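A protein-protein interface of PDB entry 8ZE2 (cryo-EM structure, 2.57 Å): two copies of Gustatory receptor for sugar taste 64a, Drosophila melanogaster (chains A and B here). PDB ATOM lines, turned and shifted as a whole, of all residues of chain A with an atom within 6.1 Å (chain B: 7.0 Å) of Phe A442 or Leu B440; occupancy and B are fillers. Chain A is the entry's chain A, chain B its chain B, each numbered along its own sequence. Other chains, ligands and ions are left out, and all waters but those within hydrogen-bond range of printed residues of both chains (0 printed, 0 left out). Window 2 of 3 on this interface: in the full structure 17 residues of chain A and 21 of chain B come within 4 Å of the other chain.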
ATOM      1  N   TYR A 435     -13.764  -4.663  22.470  1.00  0.00           N
ATOM      2  CA  TYR A 435     -15.201  -4.726  22.237  1.00  0.00           C
ATOM      3  C   TYR A 435     -15.523  -5.693  21.111  1.00  0.00           C
ATOM      4  O   TYR A 435     -16.487  -6.453  21.196  1.00  0.00           O
ATOM      5  CB  TYR A 435     -15.752  -3.333  21.929  1.00  0.00           C
ATOM      6  CG  TYR A 435     -15.826  -2.410  23.128  1.00  0.00           C
ATOM      7  CD1 TYR A 435     -15.399  -2.827  24.382  1.00  0.00           C
ATOM      8  CD2 TYR A 435     -16.337  -1.125  23.007  1.00  0.00           C
ATOM      9  CE1 TYR A 435     -15.469  -1.988  25.477  1.00  0.00           C
ATOM     10  CE2 TYR A 435     -16.412  -0.279  24.097  1.00  0.00           C
ATOM     11  CZ  TYR A 435     -15.978  -0.717  25.329  1.00  0.00           C
ATOM     12  OH  TYR A 435     -16.048   0.121  26.418  1.00  0.00           O
ATOM     13  N   VAL A 438     -15.161  -9.290  22.240  1.00  0.00           N
ATOM     14  CA  VAL A 438     -16.322  -9.830  22.949  1.00  0.00           C
ATOM     15  C   VAL A 438     -17.570  -9.855  22.057  1.00  0.00           C
ATOM     16  O   VAL A 438     -18.499 -10.629  22.311  1.00  0.00           O
ATOM     17  CB  VAL A 438     -16.577  -9.062  24.259  1.00  0.00           C
ATOM     18  CG1 VAL A 438     -15.444  -9.310  25.243  1.00  0.00           C
ATOM     19  CG2 VAL A 438     -16.747  -7.583  24.004  1.00  0.00           C
ATOM     20  N   LEU A 439     -17.612  -9.045  20.994  1.00  0.00           N
ATOM     21  CA  LEU A 439     -18.819  -8.959  20.175  1.00  0.00           C
ATOM     22  C   LEU A 439     -18.901 -10.067  19.127  1.00  0.00           C
ATOM     23  O   LEU A 439     -19.985 -10.611  18.896  1.00  0.00           O
ATOM     24  CB  LEU A 439     -18.914  -7.583  19.514  1.00  0.00           C
ATOM     25  CG  LEU A 439     -19.432  -6.470  20.432  1.00  0.00           C
ATOM     26  CD1 LEU A 439     -19.166  -5.092  19.840  1.00  0.00           C
ATOM     27  CD2 LEU A 439     -20.913  -6.658  20.720  1.00  0.00           C
ATOM     28  N   LEU A 440     -17.788 -10.424  18.481  1.00  0.00           N
ATOM     29  CA  LEU A 440     -17.848 -11.612  17.630  1.00  0.00           C
ATOM     30  C   LEU A 440     -18.109 -12.883  18.425  1.00  0.00           C
ATOM     31  O   LEU A 440     -18.416 -13.915  17.820  1.00  0.00           O
ATOM     32  CB  LEU A 440     -16.591 -11.813  16.764  1.00  0.00           C
ATOM     33  CG  LEU A 440     -16.007 -10.792  15.771  1.00  0.00           C
ATOM     34  CD1 LEU A 440     -17.097 -10.240  14.849  1.00  0.00           C
ATOM     35  CD2 LEU A 440     -15.166  -9.686  16.366  1.00  0.00           C
ATOM     36  N   GLN A 441     -17.985 -12.843  19.751  1.00  0.00           N
ATOM     37  CA  GLN A 441     -18.571 -13.885  20.584  1.00  0.00           C
ATOM     38  C   GLN A 441     -20.036 -13.610  20.897  1.00  0.00           C
ATOM     39  O   GLN A 441     -20.809 -14.557  21.088  1.00  0.00           O
ATOM     40  CB  GLN A 441     -17.785 -14.036  21.889  1.00  0.00           C
ATOM     41  CG  GLN A 441     -16.282 -13.929  21.725  1.00  0.00           C
ATOM     42  CD  GLN A 441     -15.526 -14.626  22.838  1.00  0.00           C
ATOM     43  OE1 GLN A 441     -15.044 -13.987  23.772  1.00  0.00           O
ATOM     44  NE2 GLN A 441     -15.418 -15.947  22.744  1.00  0.00           N
ATOM     45  N   PHE A 442     -20.431 -12.334  20.956  1.00  0.00           N
ATOM     46  CA  PHE A 442     -21.843 -11.999  21.123  1.00  0.00           C
ATOM     47  C   PHE A 442     -22.667 -12.488  19.938  1.00  0.00           C
ATOM     48  O   PHE A 442     -23.719 -13.113  20.113  1.00  0.00           O
ATOM     49  CB  PHE A 442     -22.010 -10.488  21.291  1.00  0.00           C
ATOM     50  CG  PHE A 442     -22.187 -10.046  22.711  1.00  0.00           C
ATOM     51  CD1 PHE A 442     -23.352 -10.337  23.401  1.00  0.00           C
ATOM     52  CD2 PHE A 442     -21.199  -9.321  23.351  1.00  0.00           C
ATOM     53  CE1 PHE A 442     -23.520  -9.925  24.707  1.00  0.00           C
ATOM     54  CE2 PHE A 442     -21.362  -8.907  24.654  1.00  0.00           C
ATOM     55  CZ  PHE A 442     -22.524  -9.208  25.335  1.00  0.00           C
ATOM     56  N   ASP A 443     -22.200 -12.212  18.719  1.00  0.00           N
ATOM     57  CA  ASP A 443     -22.928 -12.559  17.505  1.00  0.00           C
ATOM     58  C   ASP A 443     -22.307 -13.742  16.770  1.00  0.00           C
ATOM     59  O   ASP A 443     -22.488 -13.876  15.555  1.00  0.00           O
ATOM     60  CB  ASP A 443     -23.029 -11.344  16.579  1.00  0.00           C
ATOM     61  CG  ASP A 443     -21.678 -10.878  16.067  1.00  0.00           C
ATOM     62  OD1 ASP A 443     -21.130 -11.510  15.141  1.00  0.00           O
ATOM     63  OD2 ASP A 443     -21.165  -9.869  16.589  1.00  0.00           O
ATOM     64  N   GLU A 444     -21.581 -14.603  17.482  1.00  0.00           N
ATOM     65  CA  GLU A 444     -20.989 -15.779  16.845  1.00  0.00           C
ATOM     66  C   GLU A 444     -22.028 -16.708  16.227  1.00  0.00           C
ATOM     67  O   GLU A 444     -21.862 -17.083  15.054  1.00  0.00           O
ATOM     68  CB  GLU A 444     -20.108 -16.524  17.854  1.00  0.00           C
ATOM     69  CG  GLU A 444     -19.460 -17.781  17.300  1.00  0.00           C
ATOM     70  CD  GLU A 444     -18.536 -17.492  16.131  1.00  0.00           C
ATOM     71  OE1 GLU A 444     -17.847 -16.451  16.158  1.00  0.00           O
ATOM     72  OE2 GLU A 444     -18.501 -18.306  15.185  1.00  0.00           O
ATOM     73  N   PRO A 445     -23.097 -17.121  16.924  1.00  0.00           N
ATOM     74  CA  PRO A 445     -24.052 -18.046  16.291  1.00  0.00           C
ATOM     75  C   PRO A 445     -24.865 -17.419  15.171  1.00  0.00           C
ATOM     76  O   PRO A 445     -25.416 -18.158  14.346  1.00  0.00           O
ATOM     77  CB  PRO A 445     -24.956 -18.486  17.454  1.00  0.00           C
ATOM     78  CG  PRO A 445     -24.292 -17.990  18.701  1.00  0.00           C
ATOM     79  CD  PRO A 445     -23.506 -16.795  18.300  1.00  0.00           C
ATOM     80  N   ASN A 446     -24.959 -16.089  15.111  1.00  0.00           N
ATOM     81  CA  ASN A 446     -25.752 -15.455  14.061  1.00  0.00           C
ATOM     82  C   ASN A 446     -25.052 -15.531  12.710  1.00  0.00           C
ATOM     83  O   ASN A 446     -25.698 -15.780  11.685  1.00  0.00           O
ATOM     84  CB  ASN A 446     -26.053 -14.004  14.437  1.00  0.00           C
ATOM     85  CG  ASN A 446     -26.365 -13.838  15.911  1.00  0.00           C
ATOM     86  OD1 ASN A 446     -25.552 -14.174  16.771  1.00  0.00           O
ATOM     87  ND2 ASN A 446     -27.550 -13.320  16.209  1.00  0.00           N
ATOM     88  N   LEU B 338     -28.284  -2.905  34.620  1.00  0.00           N
ATOM     89  CA  LEU B 338     -27.848  -2.990  33.233  1.00  0.00           C
ATOM     90  C   LEU B 338     -27.753  -4.439  32.776  1.00  0.00           C
ATOM     91  O   LEU B 338     -27.966  -4.733  31.594  1.00  0.00           O
ATOM     92  CB  LEU B 338     -26.505  -2.278  33.063  1.00  0.00           C
ATOM     93  CG  LEU B 338     -26.572  -0.748  33.032  1.00  0.00           C
ATOM     94  CD1 LEU B 338     -25.186  -0.144  33.143  1.00  0.00           C
ATOM     95  CD2 LEU B 338     -27.258  -0.263  31.769  1.00  0.00           C
ATOM     96  N   LEU B 339     -27.433  -5.353  33.696  1.00  0.00           N
ATOM     97  CA  LEU B 339     -27.582  -6.778  33.429  1.00  0.00           C
ATOM     98  C   LEU B 339     -29.029  -7.135  33.137  1.00  0.00           C
ATOM     99  O   LEU B 339     -29.300  -8.105  32.420  1.00  0.00           O
ATOM    100  CB  LEU B 339     -27.067  -7.585  34.623  1.00  0.00           C
ATOM    101  CG  LEU B 339     -26.587  -9.018  34.407  1.00  0.00           C
ATOM    102  CD1 LEU B 339     -25.349  -9.294  35.234  1.00  0.00           C
ATOM    103  CD2 LEU B 339     -27.698  -9.984  34.783  1.00  0.00           C
ATOM    104  N   ASN B 340     -29.968  -6.364  33.681  1.00  0.00           N
ATOM    105  CA  ASN B 340     -31.389  -6.589  33.475  1.00  0.00           C
ATOM    106  C   ASN B 340     -31.991  -5.636  32.449  1.00  0.00           C
ATOM    107  O   ASN B 340     -33.215  -5.493  32.399  1.00  0.00           O
ATOM    108  CB  ASN B 340     -32.137  -6.468  34.804  1.00  0.00           C
ATOM    109  CG  ASN B 340     -32.077  -7.743  35.624  1.00  0.00           C
ATOM    110  OD1 ASN B 340     -32.329  -8.834  35.114  1.00  0.00           O
ATOM    111  ND2 ASN B 340     -31.744  -7.609  36.902  1.00  0.00           N
ATOM    112  N   VAL B 341     -31.161  -4.977  31.638  1.00  0.00           N
ATOM    113  CA  VAL B 341     -31.685  -4.064  30.624  1.00  0.00           C
ATOM    114  C   VAL B 341     -32.379  -4.845  29.515  1.00  0.00           C
ATOM    115  O   VAL B 341     -33.519  -4.549  29.140  1.00  0.00           O
ATOM    116  CB  VAL B 341     -30.559  -3.179  30.061  1.00  0.00           C
ATOM    117  CG1 VAL B 341     -30.890  -2.727  28.647  1.00  0.00           C
ATOM    118  CG2 VAL B 341     -30.342  -1.982  30.943  1.00  0.00           C
ATOM    119  N   PHE B 342     -31.703  -5.859  28.982  1.00  0.00           N
ATOM    120  CA  PHE B 342     -32.169  -6.560  27.789  1.00  0.00           C
ATOM    121  C   PHE B 342     -32.931  -7.824  28.187  1.00  0.00           C
ATOM    122  O   PHE B 342     -32.546  -8.951  27.875  1.00  0.00           O
ATOM    123  CB  PHE B 342     -30.992  -6.874  26.868  1.00  0.00           C
ATOM    124  CG  PHE B 342     -30.016  -5.740  26.723  1.00  0.00           C
ATOM    125  CD1 PHE B 342     -30.201  -4.770  25.751  1.00  0.00           C
ATOM    126  CD2 PHE B 342     -28.913  -5.643  27.556  1.00  0.00           C
ATOM    127  CE1 PHE B 342     -29.304  -3.726  25.613  1.00  0.00           C
ATOM    128  CE2 PHE B 342     -28.015  -4.601  27.425  1.00  0.00           C
ATOM    129  CZ  PHE B 342     -28.211  -3.641  26.451  1.00  0.00           C
ATOM    130  N   VAL B 433     -19.244  -1.033  30.940  1.00  0.00           N
ATOM    131  CA  VAL B 433     -19.553  -1.503  29.592  1.00  0.00           C
ATOM    132  C   VAL B 433     -18.901  -2.857  29.339  1.00  0.00           C
ATOM    133  O   VAL B 433     -19.533  -3.781  28.819  1.00  0.00           O
ATOM    134  CB  VAL B 433     -19.120  -0.460  28.545  1.00  0.00           C
ATOM    135  CG1 VAL B 433     -19.004  -1.100  27.172  1.00  0.00           C
ATOM    136  CG2 VAL B 433     -20.108   0.694  28.508  1.00  0.00           C
ATOM    137  N   THR B 434     -17.626  -2.999  29.714  1.00  0.00           N
ATOM    138  CA  THR B 434     -16.942  -4.280  29.538  1.00  0.00           C
ATOM    139  C   THR B 434     -17.553  -5.365  30.421  1.00  0.00           C
ATOM    140  O   THR B 434     -17.715  -6.517  29.988  1.00  0.00           O
ATOM    141  CB  THR B 434     -15.452  -4.125  29.841  1.00  0.00           C
ATOM    142  OG1 THR B 434     -15.284  -3.557  31.146  1.00  0.00           O
ATOM    143  CG2 THR B 434     -14.793  -3.219  28.814  1.00  0.00           C
ATOM    144  N   TYR B 435     -17.894  -5.015  31.663  1.00  0.00           N
ATOM    145  CA  TYR B 435     -18.532  -5.974  32.554  1.00  0.00           C
ATOM    146  C   TYR B 435     -19.857  -6.447  31.979  1.00  0.00           C
ATOM    147  O   TYR B 435     -20.185  -7.631  32.057  1.00  0.00           O
ATOM    148  CB  TYR B 435     -18.733  -5.360  33.941  1.00  0.00           C
ATOM    149  CG  TYR B 435     -17.462  -5.215  34.751  1.00  0.00           C
ATOM    150  CD1 TYR B 435     -16.233  -5.598  34.231  1.00  0.00           C
ATOM    151  CD2 TYR B 435     -17.494  -4.702  36.041  1.00  0.00           C
ATOM    152  CE1 TYR B 435     -15.072  -5.469  34.969  1.00  0.00           C
ATOM    153  CE2 TYR B 435     -16.339  -4.571  36.788  1.00  0.00           C
ATOM    154  CZ  TYR B 435     -15.130  -4.957  36.246  1.00  0.00           C
ATOM    155  OH  TYR B 435     -13.976  -4.826  36.984  1.00  0.00           O
ATOM    156  N   GLU B 436     -20.629  -5.540  31.382  1.00  0.00           N
ATOM    157  CA  GLU B 436     -21.858  -5.956  30.718  1.00  0.00           C
ATOM    158  C   GLU B 436     -21.553  -6.826  29.504  1.00  0.00           C
ATOM    159  O   GLU B 436     -22.211  -7.845  29.279  1.00  0.00           O
ATOM    160  CB  GLU B 436     -22.672  -4.727  30.312  1.00  0.00           C
ATOM    161  CG  GLU B 436     -23.510  -4.131  31.436  1.00  0.00           C
ATOM    162  CD  GLU B 436     -24.442  -5.135  32.087  1.00  0.00           C
ATOM    163  OE1 GLU B 436     -24.647  -5.041  33.313  1.00  0.00           O
ATOM    164  OE2 GLU B 436     -24.982  -6.008  31.377  1.00  0.00           O
ATOM    165  N   LEU B 437     -20.537  -6.455  28.723  1.00  0.00           N
ATOM    166  CA  LEU B 437     -20.198  -7.234  27.537  1.00  0.00           C
ATOM    167  C   LEU B 437     -19.804  -8.658  27.899  1.00  0.00           C
ATOM    168  O   LEU B 437     -19.920  -9.564  27.067  1.00  0.00           O
ATOM    169  CB  LEU B 437     -19.075  -6.548  26.759  1.00  0.00           C
ATOM    170  CG  LEU B 437     -19.454  -5.261  26.022  1.00  0.00           C
ATOM    171  CD1 LEU B 437     -18.213  -4.543  25.531  1.00  0.00           C
ATOM    172  CD2 LEU B 437     -20.395  -5.553  24.865  1.00  0.00           C
ATOM    173  N   VAL B 438     -19.326  -8.879  29.124  1.00  0.00           N
ATOM    174  CA  VAL B 438     -19.083 -10.261  29.533  1.00  0.00           C
ATOM    175  C   VAL B 438     -20.283 -10.848  30.288  1.00  0.00           C
ATOM    176  O   VAL B 438     -20.445 -12.072  30.342  1.00  0.00           O
ATOM    177  CB  VAL B 438     -17.785 -10.376  30.353  1.00  0.00           C
ATOM    178  CG1 VAL B 438     -16.579 -10.074  29.476  1.00  0.00           C
ATOM    179  CG2 VAL B 438     -17.812  -9.460  31.555  1.00  0.00           C
ATOM    180  N   LEU B 439     -21.153 -10.008  30.856  1.00  0.00           N
ATOM    181  CA  LEU B 439     -22.253 -10.519  31.673  1.00  0.00           C
ATOM    182  C   LEU B 439     -23.459 -10.941  30.838  1.00  0.00           C
ATOM    183  O   LEU B 439     -24.082 -11.966  31.136  1.00  0.00           O
ATOM    184  CB  LEU B 439     -22.658  -9.483  32.722  1.00  0.00           C
ATOM    185  CG  LEU B 439     -21.745  -9.429  33.952  1.00  0.00           C
ATOM    186  CD1 LEU B 439     -21.983  -8.166  34.767  1.00  0.00           C
ATOM    187  CD2 LEU B 439     -21.927 -10.671  34.810  1.00  0.00           C
ATOM    188  N   LEU B 440     -23.815 -10.187  29.794  1.00  0.00           N
ATOM    189  CA  LEU B 440     -24.844 -10.711  28.896  1.00  0.00           C
ATOM    190  C   LEU B 440     -24.393 -11.970  28.168  1.00  0.00           C
ATOM    191  O   LEU B 440     -25.233 -12.646  27.566  1.00  0.00           O
ATOM    192  CB  LEU B 440     -25.339  -9.685  27.861  1.00  0.00           C
ATOM    193  CG  LEU B 440     -25.927  -8.298  28.176  1.00  0.00           C
ATOM    194  CD1 LEU B 440     -27.008  -8.394  29.256  1.00  0.00           C
ATOM    195  CD2 LEU B 440     -24.932  -7.201  28.479  1.00  0.00           C
ATOM    196  N   GLN B 441     -23.101 -12.295  28.195  1.00  0.00           N
ATOM    197  CA  GLN B 441     -22.667 -13.644  27.857  1.00  0.00           C
ATOM    198  C   GLN B 441     -22.740 -14.585  29.052  1.00  0.00           C
ATOM    199  O   GLN B 441     -22.948 -15.790  28.870  1.00  0.00           O
ATOM    200  CB  GLN B 441     -21.241 -13.626  27.301  1.00  0.00           C
ATOM    201  CG  GLN B 441     -20.950 -12.462  26.374  1.00  0.00           C
ATOM    202  CD  GLN B 441     -19.809 -12.752  25.420  1.00  0.00           C
ATOM    203  OE1 GLN B 441     -18.679 -12.316  25.634  1.00  0.00           O
ATOM    204  NE2 GLN B 441     -20.101 -13.495  24.358  1.00  0.00           N
ATOM    205  N   PHE B 442     -22.571 -14.059  30.269  1.00  0.00           N
ATOM    206  CA  PHE B 442     -22.756 -14.876  31.466  1.00  0.00           C
ATOM    207  C   PHE B 442     -24.193 -15.370  31.576  1.00  0.00           C
ATOM    208  O   PHE B 442     -24.437 -16.558  31.818  1.00  0.00           O
ATOM    209  CB  PHE B 442     -22.378 -14.076  32.714  1.00  0.00           C
ATOM    210  CG  PHE B 442     -21.011 -14.384  33.247  1.00  0.00           C
ATOM    211  CD1 PHE B 442     -20.744 -15.604  33.844  1.00  0.00           C
ATOM    212  CD2 PHE B 442     -20.000 -13.444  33.171  1.00  0.00           C
ATOM    213  CE1 PHE B 442     -19.489 -15.886  34.340  1.00  0.00           C
ATOM    214  CE2 PHE B 442     -18.744 -13.719  33.667  1.00  0.00           C
ATOM    215  CZ  PHE B 442     -18.486 -14.942  34.252  1.00  0.00           C
ATOM    216  N   ASP B 443     -25.160 -14.469  31.400  1.00  0.00           N
ATOM    217  CA  ASP B 443     -26.572 -14.796  31.551  1.00  0.00           C
ATOM    218  C   ASP B 443     -27.299 -14.883  30.212  1.00  0.00           C
ATOM    219  O   ASP B 443     -28.518 -14.694  30.159  1.00  0.00           O
ATOM    220  CB  ASP B 443     -27.258 -13.781  32.470  1.00  0.00           C
ATOM    221  CG  ASP B 443     -27.275 -12.378  31.890  1.00  0.00           C
ATOM    222  OD1 ASP B 443     -28.104 -12.099  30.999  1.00  0.00           O
ATOM    223  OD2 ASP B 443     -26.459 -11.546  32.334  1.00  0.00           O
ATOM    224  N   GLU B 444     -26.572 -15.167  29.131  1.00  0.00           N
ATOM    225  CA  GLU B 444     -27.213 -15.303  27.824  1.00  0.00           C
ATOM    226  C   GLU B 444     -28.254 -16.415  27.782  1.00  0.00           C
ATOM    227  O   GLU B 444     -29.379 -16.155  27.321  1.00  0.00           O
ATOM    228  CB  GLU B 444     -26.143 -15.504  26.744  1.00  0.00           C
ATOM    229  CG  GLU B 444     -26.704 -15.679  25.343  1.00  0.00           C
ATOM    230  CD  GLU B 444     -27.492 -14.470  24.876  1.00  0.00           C
ATOM    231  OE1 GLU B 444     -27.086 -13.332  25.197  1.00  0.00           O
ATOM    232  OE2 GLU B 444     -28.518 -14.656  24.188  1.00  0.00           O
ATOM    233  N   PRO B 445     -27.975 -17.649  28.224  1.00  0.00           N
ATOM    234  CA  PRO B 445     -29.007 -18.696  28.129  1.00  0.00           C
ATOM    235  C   PRO B 445     -30.182 -18.488  29.069  1.00  0.00           C
ATOM    236  O   PRO B 445     -31.246 -19.073  28.835  1.00  0.00           O
ATOM    237  CB  PRO B 445     -28.244 -19.988  28.471  1.00  0.00           C
ATOM    238  CG  PRO B 445     -26.793 -19.620  28.474  1.00  0.00           C
ATOM    239  CD  PRO B 445     -26.736 -18.177  28.822  1.00  0.00           C
ATOM    240  N   ARG B 447     -31.836 -15.544  29.738  1.00  0.00           N
ATOM    241  CA  ARG B 447     -32.811 -14.671  29.094  1.00  0.00           C
ATOM    242  C   ARG B 447     -33.147 -15.172  27.694  1.00  0.00           C
ATOM    243  O   ARG B 447     -34.161 -14.784  27.113  1.00  0.00           O
ATOM    244  CB  ARG B 447     -32.295 -13.233  29.026  1.00  0.00           C
ATOM    245  CG  ARG B 447     -31.415 -12.825  30.196  1.00  0.00           C
ATOM    246  CD  ARG B 447     -31.148 -11.328  30.184  1.00  0.00           C
ATOM    247  NE  ARG B 447     -31.076 -10.792  28.830  1.00  0.00           N
ATOM    248  CZ  ARG B 447     -29.974 -10.769  28.090  1.00  0.00           C
ATOM    249  NH1 ARG B 447     -28.826 -11.245  28.544  1.00  0.00           N
ATOM    250  NH2 ARG B 447     -30.028 -10.256  26.865  1.00  0.00           N
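Of the 10 printed residues of chain A, 4 touch a printed residue of chain B.
Hydrophobic or aromatic side chains of chain A within 4 Å of the printed part of chain B: Tyr A435, Val A438 and Phe A442.
Printed residues of chain B that touch a printed residue of chain A: Val B433, Thr B434, Leu B437, Leu B440 and Gln B441.
Hydrophobic or aromatic side chains of chain B that line the printed part of chain A: Val B433, Leu B437 and Leu B440.
Along chain B the printed residues that touch a printed residue of chain A span positions 433 to 441.
Among the printed residues, 9 pairs touch across the chains.
Among the printed residues, no Asp or Glu carboxylate lies within 4 Å of a Lys or Arg side-chain nitrogen of the other chain.
Of the printed residues of chain B, Val A438 touches Leu B437 and Gln B441.
Leu A440 touches none of the printed residues of chain B.
Phe A442 touches just these residues of chain B: Leu B437 (2.9 Å), Leu B440 (3.6 Å) and Gln B441 (3.6 Å).
Phe B342 touches none of the printed residues of chain A.
Of chain A, only Phe A442 (3.6 Å) comes within 4 Å of Leu B440.
Of the printed residues of chain A, Gln B441 touches Val A438 (3.7 Å), Gln A441 (3.4 Å) and Phe A442 (3.6 Å).
The nearest printed residue of chain A that does not touch Leu B440 is Gln A441 (8.1 Å).
The nearest printed residue of chain A that does not touch Thr B434 is Val A438 (6.0 Å).
Among the printed residues, merely in contact across the chains: Phe A442 with Leu B437 (2.9 Å), Tyr A435 with Val B433 (3.3 Å), Gln A441 with Gln B441 (3.4 Å), Tyr A435 with Leu B437 (3.5 Å), Phe A442 with Gln B441 (3.6 Å), Tyr A435 with Thr B434 (3.6 Å), Phe A442 with Leu B440 (3.6 Å), Val A438 with Leu B437 (3.7 Å) and Val A438 with Gln B441 (3.7 Å).
Val A438 touches Gln B441, but with the chains exchanged Gln A441 does not touch Val B438 (7.1 Å).
Gln B441 touches its own counterpart, Gln A441.
Phe A442 touches Leu B440, but with the chains exchanged Leu A440 does not touch Phe B442 (12.7 Å).
Phe A442 touches Gln B441, but with the chains exchanged Gln A441 does not touch Phe B442 (9.4 Å).
The side-chain amide oxygen of Gln B441 sits close to the backbone carbonyl oxygen of Leu B437, 3.3 Å away.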
